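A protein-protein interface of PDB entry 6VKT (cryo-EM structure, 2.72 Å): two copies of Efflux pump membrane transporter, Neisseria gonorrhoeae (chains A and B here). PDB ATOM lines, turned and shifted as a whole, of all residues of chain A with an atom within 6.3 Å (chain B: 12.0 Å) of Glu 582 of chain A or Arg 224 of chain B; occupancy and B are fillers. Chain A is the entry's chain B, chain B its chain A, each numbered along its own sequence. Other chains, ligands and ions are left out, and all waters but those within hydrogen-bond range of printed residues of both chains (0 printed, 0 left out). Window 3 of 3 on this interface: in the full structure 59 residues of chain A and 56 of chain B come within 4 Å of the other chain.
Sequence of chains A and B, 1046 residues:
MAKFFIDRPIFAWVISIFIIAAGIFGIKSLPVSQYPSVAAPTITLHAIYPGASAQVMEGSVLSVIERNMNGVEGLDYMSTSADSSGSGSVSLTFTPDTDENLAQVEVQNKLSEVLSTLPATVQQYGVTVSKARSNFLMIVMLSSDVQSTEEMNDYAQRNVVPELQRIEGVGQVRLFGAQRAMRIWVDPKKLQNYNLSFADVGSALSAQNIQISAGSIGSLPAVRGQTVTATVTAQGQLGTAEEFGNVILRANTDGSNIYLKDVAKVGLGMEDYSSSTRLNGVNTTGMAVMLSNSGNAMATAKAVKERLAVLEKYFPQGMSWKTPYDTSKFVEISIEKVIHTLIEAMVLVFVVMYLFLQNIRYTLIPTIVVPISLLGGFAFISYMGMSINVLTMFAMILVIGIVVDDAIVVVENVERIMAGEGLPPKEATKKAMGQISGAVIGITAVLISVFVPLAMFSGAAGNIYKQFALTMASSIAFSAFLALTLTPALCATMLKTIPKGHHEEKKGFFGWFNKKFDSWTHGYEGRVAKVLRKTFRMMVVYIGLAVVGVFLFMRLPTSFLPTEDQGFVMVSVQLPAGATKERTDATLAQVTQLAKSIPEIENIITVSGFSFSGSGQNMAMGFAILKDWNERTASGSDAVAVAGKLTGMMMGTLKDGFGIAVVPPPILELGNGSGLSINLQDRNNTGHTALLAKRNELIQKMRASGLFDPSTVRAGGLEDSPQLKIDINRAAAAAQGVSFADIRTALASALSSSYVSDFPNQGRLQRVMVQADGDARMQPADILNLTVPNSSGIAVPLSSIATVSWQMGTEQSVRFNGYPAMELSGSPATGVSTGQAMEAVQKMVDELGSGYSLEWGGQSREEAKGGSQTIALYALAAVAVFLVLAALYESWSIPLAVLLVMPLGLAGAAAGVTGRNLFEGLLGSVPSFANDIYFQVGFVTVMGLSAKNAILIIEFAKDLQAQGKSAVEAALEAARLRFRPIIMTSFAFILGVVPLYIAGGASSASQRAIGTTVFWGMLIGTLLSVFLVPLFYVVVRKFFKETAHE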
ATOM      1  N   THR A 580       1.333   4.949 -15.582  1.00  0.00           N
ATOM      2  CA  THR A 580       1.151   6.161 -14.796  1.00  0.00           C
ATOM      3  C   THR A 580       2.515   6.778 -14.491  1.00  0.00           C
ATOM      4  O   THR A 580       3.546   6.364 -15.027  1.00  0.00           O
ATOM      5  CB  THR A 580       0.364   5.854 -13.524  1.00  0.00           C
ATOM      6  OG1 THR A 580       1.050   4.846 -12.769  1.00  0.00           O
ATOM      7  CG2 THR A 580      -1.029   5.359 -13.869  1.00  0.00           C
ATOM      8  N   LYS A 581       2.534   7.786 -13.620  1.00  0.00           N
ATOM      9  CA  LYS A 581       3.777   8.463 -13.276  1.00  0.00           C
ATOM     10  C   LYS A 581       4.502   7.823 -12.102  1.00  0.00           C
ATOM     11  O   LYS A 581       5.686   8.105 -11.899  1.00  0.00           O
ATOM     12  CB  LYS A 581       3.510   9.936 -12.958  1.00  0.00           C
ATOM     13  CG  LYS A 581       4.671  10.859 -13.280  1.00  0.00           C
ATOM     14  CD  LYS A 581       4.415  12.274 -12.786  1.00  0.00           C
ATOM     15  CE  LYS A 581       4.559  12.370 -11.277  1.00  0.00           C
ATOM     16  NZ  LYS A 581       4.518  13.781 -10.808  1.00  0.00           N
ATOM     17  N   GLU A 582       3.827   6.974 -11.326  1.00  0.00           N
ATOM     18  CA  GLU A 582       4.502   6.283 -10.232  1.00  0.00           C
ATOM     19  C   GLU A 582       5.537   5.298 -10.763  1.00  0.00           C
ATOM     20  O   GLU A 582       6.668   5.238 -10.260  1.00  0.00           O
ATOM     21  CB  GLU A 582       3.476   5.571  -9.353  1.00  0.00           C
ATOM     22  CG  GLU A 582       4.000   5.153  -7.992  1.00  0.00           C
ATOM     23  CD  GLU A 582       2.908   4.607  -7.095  1.00  0.00           C
ATOM     24  OE1 GLU A 582       1.744   4.549  -7.541  1.00  0.00           O
ATOM     25  OE2 GLU A 582       3.214   4.233  -5.942  1.00  0.00           O
ATOM     26  N   ARG A 583       5.171   4.522 -11.784  1.00  0.00           N
ATOM     27  CA  ARG A 583       6.126   3.617 -12.409  1.00  0.00           C
ATOM     28  C   ARG A 583       7.263   4.373 -13.082  1.00  0.00           C
ATOM     29  O   ARG A 583       8.415   3.926 -13.034  1.00  0.00           O
ATOM     30  CB  ARG A 583       5.411   2.720 -13.420  1.00  0.00           C
ATOM     31  CG  ARG A 583       4.232   1.959 -12.835  1.00  0.00           C
ATOM     32  CD  ARG A 583       3.224   1.576 -13.906  1.00  0.00           C
ATOM     33  NE  ARG A 583       3.810   0.707 -14.921  1.00  0.00           N
ATOM     34  CZ  ARG A 583       3.138   0.204 -15.951  1.00  0.00           C
ATOM     35  NH1 ARG A 583       1.844   0.458 -16.090  1.00  0.00           N
ATOM     36  NH2 ARG A 583       3.759  -0.553 -16.845  1.00  0.00           N
ATOM     37  N   THR A 584       6.966   5.519 -13.698  1.00  0.00           N
ATOM     38  CA  THR A 584       8.021   6.331 -14.292  1.00  0.00           C
ATOM     39  C   THR A 584       8.968   6.864 -13.224  1.00  0.00           C
ATOM     40  O   THR A 584      10.185   6.923 -13.437  1.00  0.00           O
ATOM     41  CB  THR A 584       7.414   7.482 -15.093  1.00  0.00           C
ATOM     42  OG1 THR A 584       6.491   6.960 -16.057  1.00  0.00           O
ATOM     43  CG2 THR A 584       8.503   8.259 -15.815  1.00  0.00           C
ATOM     44  N   ASP A 585       8.432   7.248 -12.064  1.00  0.00           N
ATOM     45  CA  ASP A 585       9.285   7.712 -10.975  1.00  0.00           C
ATOM     46  C   ASP A 585      10.152   6.584 -10.434  1.00  0.00           C
ATOM     47  O   ASP A 585      11.322   6.798 -10.102  1.00  0.00           O
ATOM     48  CB  ASP A 585       8.431   8.317  -9.861  1.00  0.00           C
ATOM     49  CG  ASP A 585       7.776   9.620 -10.272  1.00  0.00           C
ATOM     50  OD1 ASP A 585       7.997  10.063 -11.418  1.00  0.00           O
ATOM     51  OD2 ASP A 585       7.040  10.202  -9.448  1.00  0.00           O
ATOM     52  N   ALA A 586       9.597   5.375 -10.337  1.00  0.00           N
ATOM     53  CA  ALA A 586      10.402   4.233  -9.912  1.00  0.00           C
ATOM     54  C   ALA A 586      11.517   3.942 -10.912  1.00  0.00           C
ATOM     55  O   ALA A 586      12.658   3.658 -10.521  1.00  0.00           O
ATOM     56  CB  ALA A 586       9.514   3.004  -9.723  1.00  0.00           C
ATOM     57  N   THR A 587      11.207   4.015 -12.208  1.00  0.00           N
ATOM     58  CA  THR A 587      12.230   3.800 -13.225  1.00  0.00           C
ATOM     59  C   THR A 587      13.303   4.881 -13.164  1.00  0.00           C
ATOM     60  O   THR A 587      14.491   4.597 -13.343  1.00  0.00           O
ATOM     61  CB  THR A 587      11.593   3.754 -14.613  1.00  0.00           C
ATOM     62  OG1 THR A 587      10.591   2.730 -14.647  1.00  0.00           O
ATOM     63  CG2 THR A 587      12.645   3.458 -15.670  1.00  0.00           C
ATOM     64  N   GLN A 617       2.852  10.592 -19.360  1.00  0.00           N
ATOM     65  CA  GLN A 617       3.171  10.051 -18.042  1.00  0.00           C
ATOM     66  C   GLN A 617       4.170   8.904 -18.126  1.00  0.00           C
ATOM     67  O   GLN A 617       4.878   8.632 -17.150  1.00  0.00           O
ATOM     68  CB  GLN A 617       1.894   9.595 -17.337  1.00  0.00           C
ATOM     69  CG  GLN A 617       0.884  10.707 -17.101  1.00  0.00           C
ATOM     70  CD  GLN A 617      -0.243  10.288 -16.179  1.00  0.00           C
ATOM     71  OE1 GLN A 617      -1.392  10.692 -16.357  1.00  0.00           O
ATOM     72  NE2 GLN A 617       0.081   9.474 -15.183  1.00  0.00           N
ATOM     73  N   GLY B 218      -7.626   8.063 -14.597  1.00  0.00           N
ATOM     74  CA  GLY B 218      -6.320   7.819 -14.024  1.00  0.00           C
ATOM     75  C   GLY B 218      -5.383   8.984 -14.258  1.00  0.00           C
ATOM     76  O   GLY B 218      -4.254   8.804 -14.725  1.00  0.00           O
ATOM     77  N   SER B 219      -5.843  10.189 -13.929  1.00  0.00           N
ATOM     78  CA  SER B 219      -5.065  11.394 -14.174  1.00  0.00           C
ATOM     79  C   SER B 219      -3.827  11.415 -13.280  1.00  0.00           C
ATOM     80  O   SER B 219      -3.608  10.534 -12.443  1.00  0.00           O
ATOM     81  CB  SER B 219      -5.927  12.634 -13.953  1.00  0.00           C
ATOM     82  OG  SER B 219      -6.725  12.909 -15.092  1.00  0.00           O
ATOM     83  N   LEU B 220      -3.010  12.445 -13.455  1.00  0.00           N
ATOM     84  CA  LEU B 220      -1.714  12.479 -12.793  1.00  0.00           C
ATOM     85  C   LEU B 220      -1.847  12.721 -11.292  1.00  0.00           C
ATOM     86  O   LEU B 220      -1.261  11.970 -10.502  1.00  0.00           O
ATOM     87  CB  LEU B 220      -0.820  13.538 -13.439  1.00  0.00           C
ATOM     88  CG  LEU B 220       0.620  13.473 -12.951  1.00  0.00           C
ATOM     89  CD1 LEU B 220       1.041  12.030 -12.933  1.00  0.00           C
ATOM     90  CD2 LEU B 220       1.511  14.249 -13.886  1.00  0.00           C
ATOM     91  N   PRO B 221      -2.597  13.741 -10.844  1.00  0.00           N
ATOM     92  CA  PRO B 221      -2.843  13.865  -9.400  1.00  0.00           C
ATOM     93  C   PRO B 221      -3.761  12.756  -8.912  1.00  0.00           C
ATOM     94  O   PRO B 221      -4.952  12.980  -8.675  1.00  0.00           O
ATOM     95  CB  PRO B 221      -3.493  15.248  -9.265  1.00  0.00           C
ATOM     96  CG  PRO B 221      -4.097  15.509 -10.597  1.00  0.00           C
ATOM     97  CD  PRO B 221      -3.179  14.868 -11.597  1.00  0.00           C
ATOM     98  N   ALA B 222      -3.213  11.554  -8.762  1.00  0.00           N
ATOM     99  CA  ALA B 222      -3.990  10.347  -8.524  1.00  0.00           C
ATOM    100  C   ALA B 222      -3.637   9.738  -7.173  1.00  0.00           C
ATOM    101  O   ALA B 222      -2.870  10.298  -6.384  1.00  0.00           O
ATOM    102  CB  ALA B 222      -3.762   9.339  -9.651  1.00  0.00           C
ATOM    103  N   VAL B 223      -4.212   8.569  -6.914  1.00  0.00           N
ATOM    104  CA  VAL B 223      -3.994   7.855  -5.667  1.00  0.00           C
ATOM    105  C   VAL B 223      -2.762   6.970  -5.803  1.00  0.00           C
ATOM    106  O   VAL B 223      -2.320   6.637  -6.905  1.00  0.00           O
ATOM    107  CB  VAL B 223      -5.232   7.024  -5.271  1.00  0.00           C
ATOM    108  CG1 VAL B 223      -6.451   7.921  -5.143  1.00  0.00           C
ATOM    109  CG2 VAL B 223      -5.478   5.922  -6.290  1.00  0.00           C
ATOM    110  N   ARG B 224      -2.199   6.586  -4.661  1.00  0.00           N
ATOM    111  CA  ARG B 224      -1.030   5.716  -4.652  1.00  0.00           C
ATOM    112  C   ARG B 224      -1.434   4.307  -5.067  1.00  0.00           C
ATOM    113  O   ARG B 224      -2.199   3.639  -4.366  1.00  0.00           O
ATOM    114  CB  ARG B 224      -0.391   5.704  -3.265  1.00  0.00           C
ATOM    115  CG  ARG B 224       0.031   7.076  -2.764  1.00  0.00           C
ATOM    116  CD  ARG B 224       1.452   7.411  -3.189  1.00  0.00           C
ATOM    117  NE  ARG B 224       1.585   7.496  -4.640  1.00  0.00           N
ATOM    118  CZ  ARG B 224       1.403   8.610  -5.341  1.00  0.00           C
ATOM    119  NH1 ARG B 224       1.113   9.746  -4.720  1.00  0.00           N
ATOM    120  NH2 ARG B 224       1.513   8.590  -6.661  1.00  0.00           N
ATOM    121  N   GLY B 225      -0.920   3.855  -6.208  1.00  0.00           N
ATOM    122  CA  GLY B 225      -1.228   2.525  -6.697  1.00  0.00           C
ATOM    123  C   GLY B 225      -1.946   2.526  -8.029  1.00  0.00           C
ATOM    124  O   GLY B 225      -2.561   1.526  -8.412  1.00  0.00           O
ATOM    125  N   GLN B 226      -1.876   3.644  -8.746  1.00  0.00           N
ATOM    126  CA  GLN B 226      -2.488   3.760 -10.062  1.00  0.00           C
ATOM    127  C   GLN B 226      -1.496   3.304 -11.123  1.00  0.00           C
ATOM    128  O   GLN B 226      -0.340   3.740 -11.130  1.00  0.00           O
ATOM    129  CB  GLN B 226      -2.930   5.200 -10.327  1.00  0.00           C
ATOM    130  CG  GLN B 226      -3.678   5.390 -11.637  1.00  0.00           C
ATOM    131  CD  GLN B 226      -4.979   4.614 -11.681  1.00  0.00           C
ATOM    132  OE1 GLN B 226      -5.078   3.583 -12.346  1.00  0.00           O
ATOM    133  NE2 GLN B 226      -5.985   5.107 -10.970  1.00  0.00           N
ATOM    134  N   THR B 227      -1.949   2.426 -12.016  1.00  0.00           N
ATOM    135  CA  THR B 227      -1.086   1.847 -13.035  1.00  0.00           C
ATOM    136  C   THR B 227      -1.574   2.059 -14.459  1.00  0.00           C
ATOM    137  O   THR B 227      -0.770   1.953 -15.387  1.00  0.00           O
ATOM    138  CB  THR B 227      -0.916   0.337 -12.798  1.00  0.00           C
ATOM    139  OG1 THR B 227      -2.204  -0.289 -12.750  1.00  0.00           O
ATOM    140  CG2 THR B 227      -0.188   0.083 -11.488  1.00  0.00           C
ATOM    141  N   VAL B 228      -2.855   2.352 -14.662  1.00  0.00           N
ATOM    142  CA  VAL B 228      -3.432   2.498 -15.993  1.00  0.00           C
ATOM    143  C   VAL B 228      -4.005   3.901 -16.132  1.00  0.00           C
ATOM    144  O   VAL B 228      -4.673   4.401 -15.219  1.00  0.00           O
ATOM    145  CB  VAL B 228      -4.513   1.436 -16.257  1.00  0.00           C
ATOM    146  CG1 VAL B 228      -5.169   1.672 -17.608  1.00  0.00           C
ATOM    147  CG2 VAL B 228      -3.911   0.042 -16.187  1.00  0.00           C
ATOM    148  N   THR B 229      -3.741   4.533 -17.273  1.00  0.00           N
ATOM    149  CA  THR B 229      -4.287   5.840 -17.612  1.00  0.00           C
ATOM    150  C   THR B 229      -4.851   5.769 -19.023  1.00  0.00           C
ATOM    151  O   THR B 229      -4.203   5.222 -19.921  1.00  0.00           O
ATOM    152  CB  THR B 229      -3.218   6.934 -17.523  1.00  0.00           C
ATOM    153  OG1 THR B 229      -2.563   6.862 -16.250  1.00  0.00           O
ATOM    154  CG2 THR B 229      -3.846   8.308 -17.689  1.00  0.00           C
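O of Thr 227 of chain B sits at hydrogen-bond distance from NH1 of Arg 583 of chain A.
The side-chain hydroxyl (OG1) of Thr 580 of chain A sits at hydrogen-bond distance from the backbone carbonyl oxygen (O) of Gln 226 of chain B (2.4 Å).
The side-chain carboxylate (OE2) of Glu 582 of chain A lies within salt-bridge range of the guanidinium group (NE) of Arg 224 of chain B, 3.9 Å away.
N of Gly 225 of chain B lies within hydrogen-bond range of OE1 of Glu 582 of chain A, at 3.1 Å.
No position is printed for both chains.
Among the printed residues, merely in contact across the chains: Thr 580 of chain A with Thr 229 of chain B (3.2 Å), Lys 581 of chain A with Leu 220 of chain B (3.2 Å), Thr 580 of chain A with Thr 227 of chain B (3.4 Å), Gln 617 of chain A with Leu 220 of chain B (3.5 Å), Thr 580 of chain A with Val 228 of chain B (3.6 Å), Gln 617 of chain A with Thr 229 of chain B (3.7 Å), Gln 617 of chain A with Gly 218 of chain B (3.8 Å), Glu 582 of chain A with Gln 226 of chain B (3.9 Å) and Gln 617 of chain A with Ser 219 of chain B (3.99 Å).
Of chain B, only Leu 220 (3.2 Å) comes within 4 Å of Lys 581 of chain A.
Of chain B, only Arg 224, Gly 225 and Gln 226 come within 4 Å of Glu 582 of chain A.
No residue of chain B comes within 4 Å of Asp 585 of chain A.
No residue of chain B comes within 4 Å of Ala 586 of chain A.
Of the printed residues of chain A, Gly 218 of chain B touches Gln 617 (3.8 Å).
Ala 222 of chain B touches none of the printed residues of chain A.
Val 223 of chain B touches none of the printed residues of chain A.
Printed residues of chain A within 4 Å of Gly 225 of chain B: Glu 582 (3.1 Å).
Printed residues of chain A within 4 Å of Val 228 of chain B: Thr 580 (3.6 Å).
The nearest residue of chain B that does not touch Glu 582 of chain A is Val 223 of chain B (4.6 Å).
The side-chain hydroxyl (OG1) of Thr 584 of chain A is in hydrogen-bond range of the backbone carbonyl oxygen (O) of Gln 617 of chain A, at 2.6 Å.
O of Thr 580 of chain A sits at hydrogen-bond distance from OG1 of Thr 584 of chain A (3.2 Å).
OE1 of Gln 226 of chain B lies close to O of Val 228 of chain B.
The side-chain hydroxyl (OG1) of Thr 587 of chain A lies within hydrogen-bond range of the backbone carbonyl oxygen (O) of Arg 583 of chain A (3.0 Å).
O of Gly 218 of chain B is in hydrogen-bond range of OG1 of Thr 229 of chain B (3.0 Å).
The backbone NH (N) of Lys 581 of chain A sits close to the side-chain amide nitrogen (NE2) of Gln 617 of chain A, 3.4 Å away.
Printed residues of chain A that touch a printed residue of chain B: Thr 580, Lys 581, Glu 582, Arg 583 and Gln 617.
Printed residues of chain B that touch a printed residue of chain A: Gly 218, Ser 219, Leu 220, Arg 224, Gly 225, Gln 226, Thr 227, Val 228 and Thr 229.
Hydrophobic or aromatic side chains of chain B that line the printed part of chain A: Leu 220.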
